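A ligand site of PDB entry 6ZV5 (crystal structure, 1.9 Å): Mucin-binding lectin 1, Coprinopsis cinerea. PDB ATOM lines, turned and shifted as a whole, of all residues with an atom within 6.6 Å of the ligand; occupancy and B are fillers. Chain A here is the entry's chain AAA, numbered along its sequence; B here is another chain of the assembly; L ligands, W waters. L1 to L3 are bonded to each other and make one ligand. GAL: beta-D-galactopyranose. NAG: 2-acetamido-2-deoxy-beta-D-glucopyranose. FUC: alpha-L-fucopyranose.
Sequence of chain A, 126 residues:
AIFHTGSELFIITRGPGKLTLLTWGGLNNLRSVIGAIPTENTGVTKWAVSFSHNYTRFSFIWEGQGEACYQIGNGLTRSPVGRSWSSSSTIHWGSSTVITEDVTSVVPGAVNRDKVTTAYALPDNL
CD1 of Leu 27 touches O5 of FUC L3, at 3.4 Å.
Tyr 55 of chain A touches the ligand.
CB of Arg 31 of chain B touches O6 of NAG L2, at 3.7 Å.
Val 111 of chain B touches the ligand.
Hydrophobic or aromatic side chains that line the ligand: Leu 27, His 53, Trp 93 and Val 111 of chain B.
Eight residues have an atom within 4 Å of the ligand: Leu 27, His 53, Asn 54, Tyr 55 of chain A, Trp 93, Arg 31 of chain B, Val 111 of chain B and Arg 113 of chain B.
Water W7 lies within hydrogen-bond range of O2 of FUC L3, OD1 of Asn 54 and O of Arg 31 of chain B.
Water W1 lies within hydrogen-bond range of an oxygen (O4) of FUC L3 (2.7 Å), the backbone carbonyl oxygen of Tyr 55 of chain A (2.8 Å) and the backbone carbonyl oxygen of Ser 52 (3.5 Å).
Water W2 bridges O3 of FUC L3 (2.7 Å) and O of Val 116 of chain B (2.9 Å).
Water W5 bridges the backbone NH of Arg 31 of chain B (2.8 Å) and an oxygen (O6) of NAG L2 (3.5 Å).
N of Leu 27 lies within hydrogen-bond range of O of Asn 54 (3.0 Å).
OH of Tyr 55 of chain B sits at hydrogen-bond distance from ND2 of Asn 54, at 3.0 Å.
The backbone NH (N) of Trp 93 lies within hydrogen-bond range of the backbone carbonyl oxygen (O) of Thr 56 (2.9 Å).
The backbone carbonyl oxygen of Arg 31 of chain B sits at hydrogen-bond distance from the side-chain hydroxyl of Tyr 55 of chain B.
N of Val 111 of chain B is in hydrogen-bond range of O of Ser 32 of chain B (2.7 Å).
An oxygen (O3) of FUC L3 lies within hydrogen-bond range of a ring nitrogen (ND1) of His 53 (2.8 Å).
An oxygen (O4) of FUC L3 sits at hydrogen-bond distance from the backbone NH (N) of Asn 54 (2.9 Å).
The indole nitrogen (NE1) of Trp 93 sits at hydrogen-bond distance from an oxygen (O4) of GAL L1 (2.9 Å).
O2 of FUC L3 lies within hydrogen-bond range of NH2 of Arg 113 of chain B.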
ATOM      1  N   HIS A   4      17.665 -28.379   2.578  1.00  0.00           N
ATOM      2  CA  HIS A   4      18.378 -28.433   3.854  1.00  0.00           C
ATOM      3  C   HIS A   4      19.386 -29.569   3.810  1.00  0.00           C
ATOM      4  O   HIS A   4      19.183 -30.585   3.050  1.00  0.00           O
ATOM      5  CB  HIS A   4      17.400 -28.567   5.033  1.00  0.00           C
ATOM      6  CG  HIS A   4      16.529 -27.351   5.241  1.00  0.00           C
ATOM      7  ND1 HIS A   4      16.311 -26.805   6.490  1.00  0.00           N
ATOM      8  CD2 HIS A   4      15.838 -26.579   4.374  1.00  0.00           C
ATOM      9  CE1 HIS A   4      15.513 -25.766   6.389  1.00  0.00           C
ATOM     10  NE2 HIS A   4      15.201 -25.594   5.086  1.00  0.00           N
ATOM     11  N   LEU A  27      11.796 -12.580  -3.351  1.00  0.00           N
ATOM     12  CA  LEU A  27      11.464 -11.502  -2.384  1.00  0.00           C
ATOM     13  C   LEU A  27      11.766 -10.122  -3.032  1.00  0.00           C
ATOM     14  O   LEU A  27      12.606 -10.046  -3.983  1.00  0.00           O
ATOM     15  CB  LEU A  27      12.291 -11.722  -1.118  1.00  0.00           C
ATOM     16  CG  LEU A  27      11.910 -12.996  -0.350  1.00  0.00           C
ATOM     17  CD1 LEU A  27      12.984 -13.411   0.671  1.00  0.00           C
ATOM     18  CD2 LEU A  27      10.566 -12.769   0.325  1.00  0.00           C
ATOM     19  N   ASN A  28      10.977  -9.127  -2.657  1.00  0.00           N
ATOM     20  CA  ASN A  28      11.114  -7.733  -3.096  1.00  0.00           C
ATOM     21  C   ASN A  28      11.394  -7.591  -4.584  1.00  0.00           C
ATOM     22  O   ASN A  28      12.324  -6.879  -4.976  1.00  0.00           O
ATOM     23  CB  ASN A  28      12.135  -7.033  -2.215  1.00  0.00           C
ATOM     24  CG  ASN A  28      11.451  -6.577  -0.923  1.00  0.00           C
ATOM     25  OD1 ASN A  28      11.827  -7.014   0.156  1.00  0.00           O
ATOM     26  ND2 ASN A  28      10.387  -5.774  -1.015  1.00  0.00           N
ATOM     27  N   PHE A  51      18.844 -24.417  -4.823  1.00  0.00           N
ATOM     28  CA  PHE A  51      18.069 -23.169  -4.743  1.00  0.00           C
ATOM     29  C   PHE A  51      19.007 -21.966  -4.871  1.00  0.00           C
ATOM     30  O   PHE A  51      20.225 -22.147  -4.921  1.00  0.00           O
ATOM     31  CB  PHE A  51      17.307 -23.133  -3.416  1.00  0.00           C
ATOM     32  CG  PHE A  51      18.109 -22.879  -2.189  1.00  0.00           C
ATOM     33  CD1 PHE A  51      18.826 -23.890  -1.576  1.00  0.00           C
ATOM     34  CD2 PHE A  51      18.131 -21.617  -1.602  1.00  0.00           C
ATOM     35  CE1 PHE A  51      19.539 -23.658  -0.415  1.00  0.00           C
ATOM     36  CE2 PHE A  51      18.832 -21.388  -0.429  1.00  0.00           C
ATOM     37  CZ  PHE A  51      19.553 -22.389   0.174  1.00  0.00           C
ATOM     38  N   SER A  52      18.445 -20.754  -4.951  1.00  0.00           N
ATOM     39  CA  SER A  52      19.163 -19.451  -4.799  1.00  0.00           C
ATOM     40  C   SER A  52      18.557 -18.780  -3.562  1.00  0.00           C
ATOM     41  O   SER A  52      17.318 -18.768  -3.432  1.00  0.00           O
ATOM     42  CB  SER A  52      19.014 -18.560  -5.939  1.00  0.00           C
ATOM     43  OG  SER A  52      19.737 -18.963  -7.101  1.00  0.00           O
ATOM     44  N   HIS A  53      19.375 -18.252  -2.679  1.00  0.00           N
ATOM     45  CA  HIS A  53      18.900 -17.449  -1.577  1.00  0.00           C
ATOM     46  C   HIS A  53      17.980 -16.312  -2.105  1.00  0.00           C
ATOM     47  O   HIS A  53      18.147 -15.809  -3.256  1.00  0.00           O
ATOM     48  CB  HIS A  53      20.030 -16.913  -0.726  1.00  0.00           C
ATOM     49  CG  HIS A  53      20.720 -17.956   0.063  1.00  0.00           C
ATOM     50  ND1 HIS A  53      20.212 -18.446   1.224  1.00  0.00           N
ATOM     51  CD2 HIS A  53      21.908 -18.554  -0.116  1.00  0.00           C
ATOM     52  CE1 HIS A  53      21.074 -19.322   1.738  1.00  0.00           C
ATOM     53  NE2 HIS A  53      22.093 -19.429   0.916  1.00  0.00           N
ATOM     54  N   ASN A  54      16.984 -16.019  -1.268  1.00  0.00           N
ATOM     55  CA  ASN A  54      15.975 -14.947  -1.466  1.00  0.00           C
ATOM     56  C   ASN A  54      14.891 -15.374  -2.460  1.00  0.00           C
ATOM     57  O   ASN A  54      14.046 -14.514  -2.774  1.00  0.00           O
ATOM     58  CB  ASN A  54      16.559 -13.625  -1.931  1.00  0.00           C
ATOM     59  CG  ASN A  54      17.727 -13.170  -1.086  1.00  0.00           C
ATOM     60  OD1 ASN A  54      17.579 -12.985   0.132  1.00  0.00           O
ATOM     61  ND2 ASN A  54      18.878 -13.001  -1.712  1.00  0.00           N
ATOM     62  N   TYR A  55      14.840 -16.633  -2.927  1.00  0.00           N
ATOM     63  CA  TYR A  55      13.688 -17.098  -3.736  1.00  0.00           C
ATOM     64  C   TYR A  55      12.897 -18.153  -2.996  1.00  0.00           C
ATOM     65  O   TYR A  55      13.463 -18.842  -2.156  1.00  0.00           O
ATOM     66  CB  TYR A  55      14.177 -17.620  -5.067  1.00  0.00           C
ATOM     67  CG  TYR A  55      14.701 -16.582  -6.001  1.00  0.00           C
ATOM     68  CD1 TYR A  55      16.021 -16.177  -5.960  1.00  0.00           C
ATOM     69  CD2 TYR A  55      13.902 -16.063  -6.995  1.00  0.00           C
ATOM     70  CE1 TYR A  55      16.527 -15.252  -6.870  1.00  0.00           C
ATOM     71  CE2 TYR A  55      14.383 -15.143  -7.891  1.00  0.00           C
ATOM     72  CZ  TYR A  55      15.699 -14.720  -7.817  1.00  0.00           C
ATOM     73  OH  TYR A  55      16.179 -13.839  -8.747  1.00  0.00           O
ATOM     74  N   THR A  56      11.593 -18.254  -3.286  1.00  0.00           N
ATOM     75  CA  THR A  56      10.666 -19.097  -2.467  1.00  0.00           C
ATOM     76  C   THR A  56      10.020 -20.177  -3.318  1.00  0.00           C
ATOM     77  O   THR A  56       9.341 -21.023  -2.723  1.00  0.00           O
ATOM     78  CB  THR A  56       9.575 -18.242  -1.789  1.00  0.00           C
ATOM     79  OG1 THR A  56       8.872 -17.571  -2.828  1.00  0.00           O
ATOM     80  CG2 THR A  56      10.152 -17.216  -0.847  1.00  0.00           C
ATOM     81  N   TRP A  93       9.485 -23.369  -1.065  1.00  0.00           N
ATOM     82  CA  TRP A  93      10.513 -23.176  -0.023  1.00  0.00           C
ATOM     83  C   TRP A  93       9.931 -23.520   1.341  1.00  0.00           C
ATOM     84  O   TRP A  93       8.890 -22.977   1.690  1.00  0.00           O
ATOM     85  CB  TRP A  93      11.112 -21.755  -0.112  1.00  0.00           C
ATOM     86  CG  TRP A  93      12.164 -21.529   0.919  1.00  0.00           C
ATOM     87  CD1 TRP A  93      12.070 -20.782   2.040  1.00  0.00           C
ATOM     88  CD2 TRP A  93      13.494 -22.089   0.899  1.00  0.00           C
ATOM     89  NE1 TRP A  93      13.279 -20.762   2.730  1.00  0.00           N
ATOM     90  CE2 TRP A  93      14.173 -21.578   2.034  1.00  0.00           C
ATOM     91  CE3 TRP A  93      14.186 -22.924   0.007  1.00  0.00           C
ATOM     92  CZ2 TRP A  93      15.477 -21.946   2.348  1.00  0.00           C
ATOM     93  CZ3 TRP A  93      15.492 -23.231   0.295  1.00  0.00           C
ATOM     94  CH2 TRP A  93      16.122 -22.770   1.445  1.00  0.00           C
ATOM     95  N   GLY A  94      10.547 -24.459   2.043  1.00  0.00           N
ATOM     96  CA  GLY A  94      10.143 -24.932   3.379  1.00  0.00           C
ATOM     97  C   GLY A  94       9.443 -26.283   3.290  1.00  0.00           C
ATOM     98  O   GLY A  94       9.365 -26.989   4.352  1.00  0.00           O
ATOM     99  N   LEU B  30      21.001  -6.758  -1.328  1.00  0.00           N
ATOM    100  CA  LEU B  30      20.691  -8.125  -0.790  1.00  0.00           C
ATOM    101  C   LEU B  30      21.637  -8.446   0.349  1.00  0.00           C
ATOM    102  O   LEU B  30      22.835  -8.118   0.273  1.00  0.00           O
ATOM    103  CB  LEU B  30      20.790  -9.168  -1.891  1.00  0.00           C
ATOM    104  CG  LEU B  30      19.642  -9.114  -2.894  1.00  0.00           C
ATOM    105  CD1 LEU B  30      19.905 -10.060  -4.059  1.00  0.00           C
ATOM    106  CD2 LEU B  30      18.309  -9.393  -2.232  1.00  0.00           C
ATOM    107  N   ARG B  31      21.113  -9.032   1.400  1.00  0.00           N
ATOM    108  CA  ARG B  31      21.908  -9.371   2.609  1.00  0.00           C
ATOM    109  C   ARG B  31      22.842 -10.544   2.228  1.00  0.00           C
ATOM    110  O   ARG B  31      22.385 -11.558   1.581  1.00  0.00           O
ATOM    111  CB  ARG B  31      20.948  -9.805   3.682  1.00  0.00           C
ATOM    112  CG  ARG B  31      21.613 -10.176   4.986  1.00  0.00           C
ATOM    113  CD  ARG B  31      21.810  -9.056   5.943  1.00  0.00           C
ATOM    114  NE  ARG B  31      22.467  -9.475   7.172  1.00  0.00           N
ATOM    115  CZ  ARG B  31      21.875  -9.799   8.304  1.00  0.00           C
ATOM    116  NH1 ARG B  31      20.552  -9.877   8.390  1.00  0.00           N
ATOM    117  NH2 ARG B  31      22.617 -10.105   9.374  1.00  0.00           N
ATOM    118  N   SER B  32      24.102 -10.440   2.629  1.00  0.00           N
ATOM    119  CA  SER B  32      25.091 -11.527   2.523  1.00  0.00           C
ATOM    120  C   SER B  32      24.666 -12.707   3.421  1.00  0.00           C
ATOM    121  O   SER B  32      24.089 -12.484   4.545  1.00  0.00           O
ATOM    122  CB  SER B  32      26.437 -10.983   2.911  1.00  0.00           C
ATOM    123  OG  SER B  32      26.930 -10.145   1.830  1.00  0.00           O
ATOM    124  N   VAL B  33      25.025 -13.928   2.998  1.00  0.00           N
ATOM    125  CA  VAL B  33      24.692 -15.177   3.727  1.00  0.00           C
ATOM    126  C   VAL B  33      25.967 -15.956   4.035  1.00  0.00           C
ATOM    127  O   VAL B  33      26.835 -16.050   3.152  1.00  0.00           O
ATOM    128  CB  VAL B  33      23.724 -16.029   2.902  1.00  0.00           C
ATOM    129  CG1 VAL B  33      23.462 -17.364   3.567  1.00  0.00           C
ATOM    130  CG2 VAL B  33      22.464 -15.263   2.590  1.00  0.00           C
ATOM    131  N   TYR B  55      23.974 -12.562  -6.791  1.00  0.00           N
ATOM    132  CA  TYR B  55      25.197 -12.308  -6.018  1.00  0.00           C
ATOM    133  C   TYR B  55      26.423 -12.377  -6.910  1.00  0.00           C
ATOM    134  O   TYR B  55      26.369 -13.104  -7.917  1.00  0.00           O
ATOM    135  CB  TYR B  55      25.287 -13.279  -4.865  1.00  0.00           C
ATOM    136  CG  TYR B  55      24.293 -13.061  -3.759  1.00  0.00           C
ATOM    137  CD1 TYR B  55      23.054 -13.631  -3.792  1.00  0.00           C
ATOM    138  CD2 TYR B  55      24.608 -12.305  -2.658  1.00  0.00           C
ATOM    139  CE1 TYR B  55      22.126 -13.445  -2.785  1.00  0.00           C
ATOM    140  CE2 TYR B  55      23.719 -12.123  -1.639  1.00  0.00           C
ATOM    141  CZ  TYR B  55      22.488 -12.750  -1.669  1.00  0.00           C
ATOM    142  OH  TYR B  55      21.633 -12.605  -0.609  1.00  0.00           O
ATOM    143  N   VAL B 111      24.078 -12.872   7.215  1.00  0.00           N
ATOM    144  CA  VAL B 111      23.083 -13.610   8.049  1.00  0.00           C
ATOM    145  C   VAL B 111      23.413 -15.112   8.084  1.00  0.00           C
ATOM    146  O   VAL B 111      23.821 -15.707   7.038  1.00  0.00           O
ATOM    147  CB  VAL B 111      21.640 -13.344   7.579  1.00  0.00           C
ATOM    148  CG1 VAL B 111      21.360 -13.865   6.167  1.00  0.00           C
ATOM    149  CG2 VAL B 111      20.642 -13.904   8.595  1.00  0.00           C
ATOM    150  N   ASN B 112      23.261 -15.743   9.230  1.00  0.00           N
ATOM    151  CA  ASN B 112      23.583 -17.179   9.417  1.00  0.00           C
ATOM    152  C   ASN B 112      22.485 -18.068   8.841  1.00  0.00           C
ATOM    153  O   ASN B 112      21.294 -17.929   9.199  1.00  0.00           O
ATOM    154  CB  ASN B 112      23.992 -17.457  10.854  1.00  0.00           C
ATOM    155  CG  ASN B 112      24.367 -18.884  11.063  1.00  0.00           C
ATOM    156  OD1 ASN B 112      23.532 -19.766  10.885  1.00  0.00           O
ATOM    157  ND2 ASN B 112      25.629 -19.142  11.386  1.00  0.00           N
ATOM    158  N   ARG B 113      22.870 -18.979   7.962  1.00  0.00           N
ATOM    159  CA  ARG B 113      21.982 -19.973   7.312  1.00  0.00           C
ATOM    160  C   ARG B 113      22.632 -21.358   7.357  1.00  0.00           C
ATOM    161  O   ARG B 113      22.612 -22.073   6.344  1.00  0.00           O
ATOM    162  CB  ARG B 113      21.646 -19.561   5.895  1.00  0.00           C
ATOM    163  CG  ARG B 113      20.977 -18.202   5.810  1.00  0.00           C
ATOM    164  CD  ARG B 113      19.606 -18.184   6.470  1.00  0.00           C
ATOM    165  NE  ARG B 113      18.907 -16.956   6.142  1.00  0.00           N
ATOM    166  CZ  ARG B 113      18.330 -16.136   7.020  1.00  0.00           C
ATOM    167  NH1 ARG B 113      18.378 -16.406   8.316  1.00  0.00           N
ATOM    168  NH2 ARG B 113      17.744 -15.054   6.573  1.00  0.00           N
ATOM    169  N   VAL B 116      21.494 -24.669   5.658  1.00  0.00           N
ATOM    170  CA  VAL B 116      20.516 -24.215   4.632  1.00  0.00           C
ATOM    171  C   VAL B 116      21.184 -23.187   3.720  1.00  0.00           C
ATOM    172  O   VAL B 116      20.611 -22.089   3.507  1.00  0.00           O
ATOM    173  CB  VAL B 116      19.207 -23.628   5.203  1.00  0.00           C
ATOM    174  CG1 VAL B 116      18.112 -23.818   4.196  1.00  0.00           C
ATOM    175  CG2 VAL B 116      18.817 -24.213   6.535  1.00  0.00           C
HETATM  176  C1  GAL L   1      12.844 -16.079   5.092  1.00  0.00           C
HETATM  177  C2  GAL L   1      12.017 -17.242   4.536  1.00  0.00           C
HETATM  178  C3  GAL L   1      11.867 -18.341   5.530  1.00  0.00           C
HETATM  179  C4  GAL L   1      13.209 -18.745   6.171  1.00  0.00           C
HETATM  180  C5  GAL L   1      13.906 -17.456   6.705  1.00  0.00           C
HETATM  181  C6  GAL L   1      15.274 -17.605   7.274  1.00  0.00           C
HETATM  182  O2  GAL L   1      10.727 -16.721   4.204  1.00  0.00           O
HETATM  183  O3  GAL L   1      11.322 -19.464   4.880  1.00  0.00           O
HETATM  184  O4  GAL L   1      14.025 -19.428   5.197  1.00  0.00           O
HETATM  185  O5  GAL L   1      14.063 -16.544   5.659  1.00  0.00           O
HETATM  186  O6  GAL L   1      15.400 -18.668   8.216  1.00  0.00           O
HETATM  187  C1  NAG L   2      13.474 -11.543   5.439  1.00  0.00           C
HETATM  188  C2  NAG L   2      12.760 -12.806   4.911  1.00  0.00           C
HETATM  189  C3  NAG L   2      13.752 -13.973   4.765  1.00  0.00           C
HETATM  190  C4  NAG L   2      14.944 -13.567   3.939  1.00  0.00           C
HETATM  191  C5  NAG L   2      15.565 -12.278   4.530  1.00  0.00           C
HETATM  192  C6  NAG L   2      16.671 -11.639   3.715  1.00  0.00           C
HETATM  193  C7  NAG L   2      10.382 -13.201   5.455  1.00  0.00           C
HETATM  194  C8  NAG L   2       9.403 -13.477   6.569  1.00  0.00           C
HETATM  195  N2  NAG L   2      11.681 -13.194   5.808  1.00  0.00           N
HETATM  196  O1  NAG L   2      12.560 -10.481   5.467  1.00  0.00           O
HETATM  197  O3  NAG L   2      13.007 -15.027   4.141  1.00  0.00           O
HETATM  198  O4  NAG L   2      15.834 -14.695   3.972  1.00  0.00           O
HETATM  199  O5  NAG L   2      14.582 -11.224   4.612  1.00  0.00           O
HETATM  200  O6  NAG L   2      17.455 -10.792   4.597  1.00  0.00           O
HETATM  201  O7  NAG L   2      10.002 -12.968   4.295  1.00  0.00           O
HETATM  202  C1  FUC L   3      16.398 -14.828   2.685  1.00  0.00           C
HETATM  203  C2  FUC L   3      17.654 -15.744   2.757  1.00  0.00           C
HETATM  204  C3  FUC L   3      17.265 -17.144   3.205  1.00  0.00           C
HETATM  205  C4  FUC L   3      16.222 -17.703   2.262  1.00  0.00           C
HETATM  206  C5  FUC L   3      15.015 -16.750   2.163  1.00  0.00           C
HETATM  207  C6  FUC L   3      14.058 -17.143   1.056  1.00  0.00           C
HETATM  208  O2  FUC L   3      18.560 -15.169   3.678  1.00  0.00           O
HETATM  209  O3  FUC L   3      18.384 -17.978   3.303  1.00  0.00           O
HETATM  210  O4  FUC L   3      16.809 -17.841   0.980  1.00  0.00           O
HETATM  211  O5  FUC L   3      15.430 -15.443   1.793  1.00  0.00           O
HETATM  212  O   HOH W   1      15.639 -19.694  -0.552  1.00  0.00           O
HETATM  213  O   HOH W   2      18.276 -20.546   4.057  1.00  0.00           O
HETATM  214  O   HOH W   3      16.545 -20.988   5.993  1.00  0.00           O
HETATM  215  O   HOH W   4      12.301 -14.021   8.325  1.00  0.00           O
HETATM  216  O   HOH W   5      18.283  -9.087   1.701  1.00  0.00           O
HETATM  217  O   HOH W   6      11.906 -22.397   5.630  1.00  0.00           O
HETATM  218  O   HOH W   7      19.620 -13.239   2.349  1.00  0.00           O
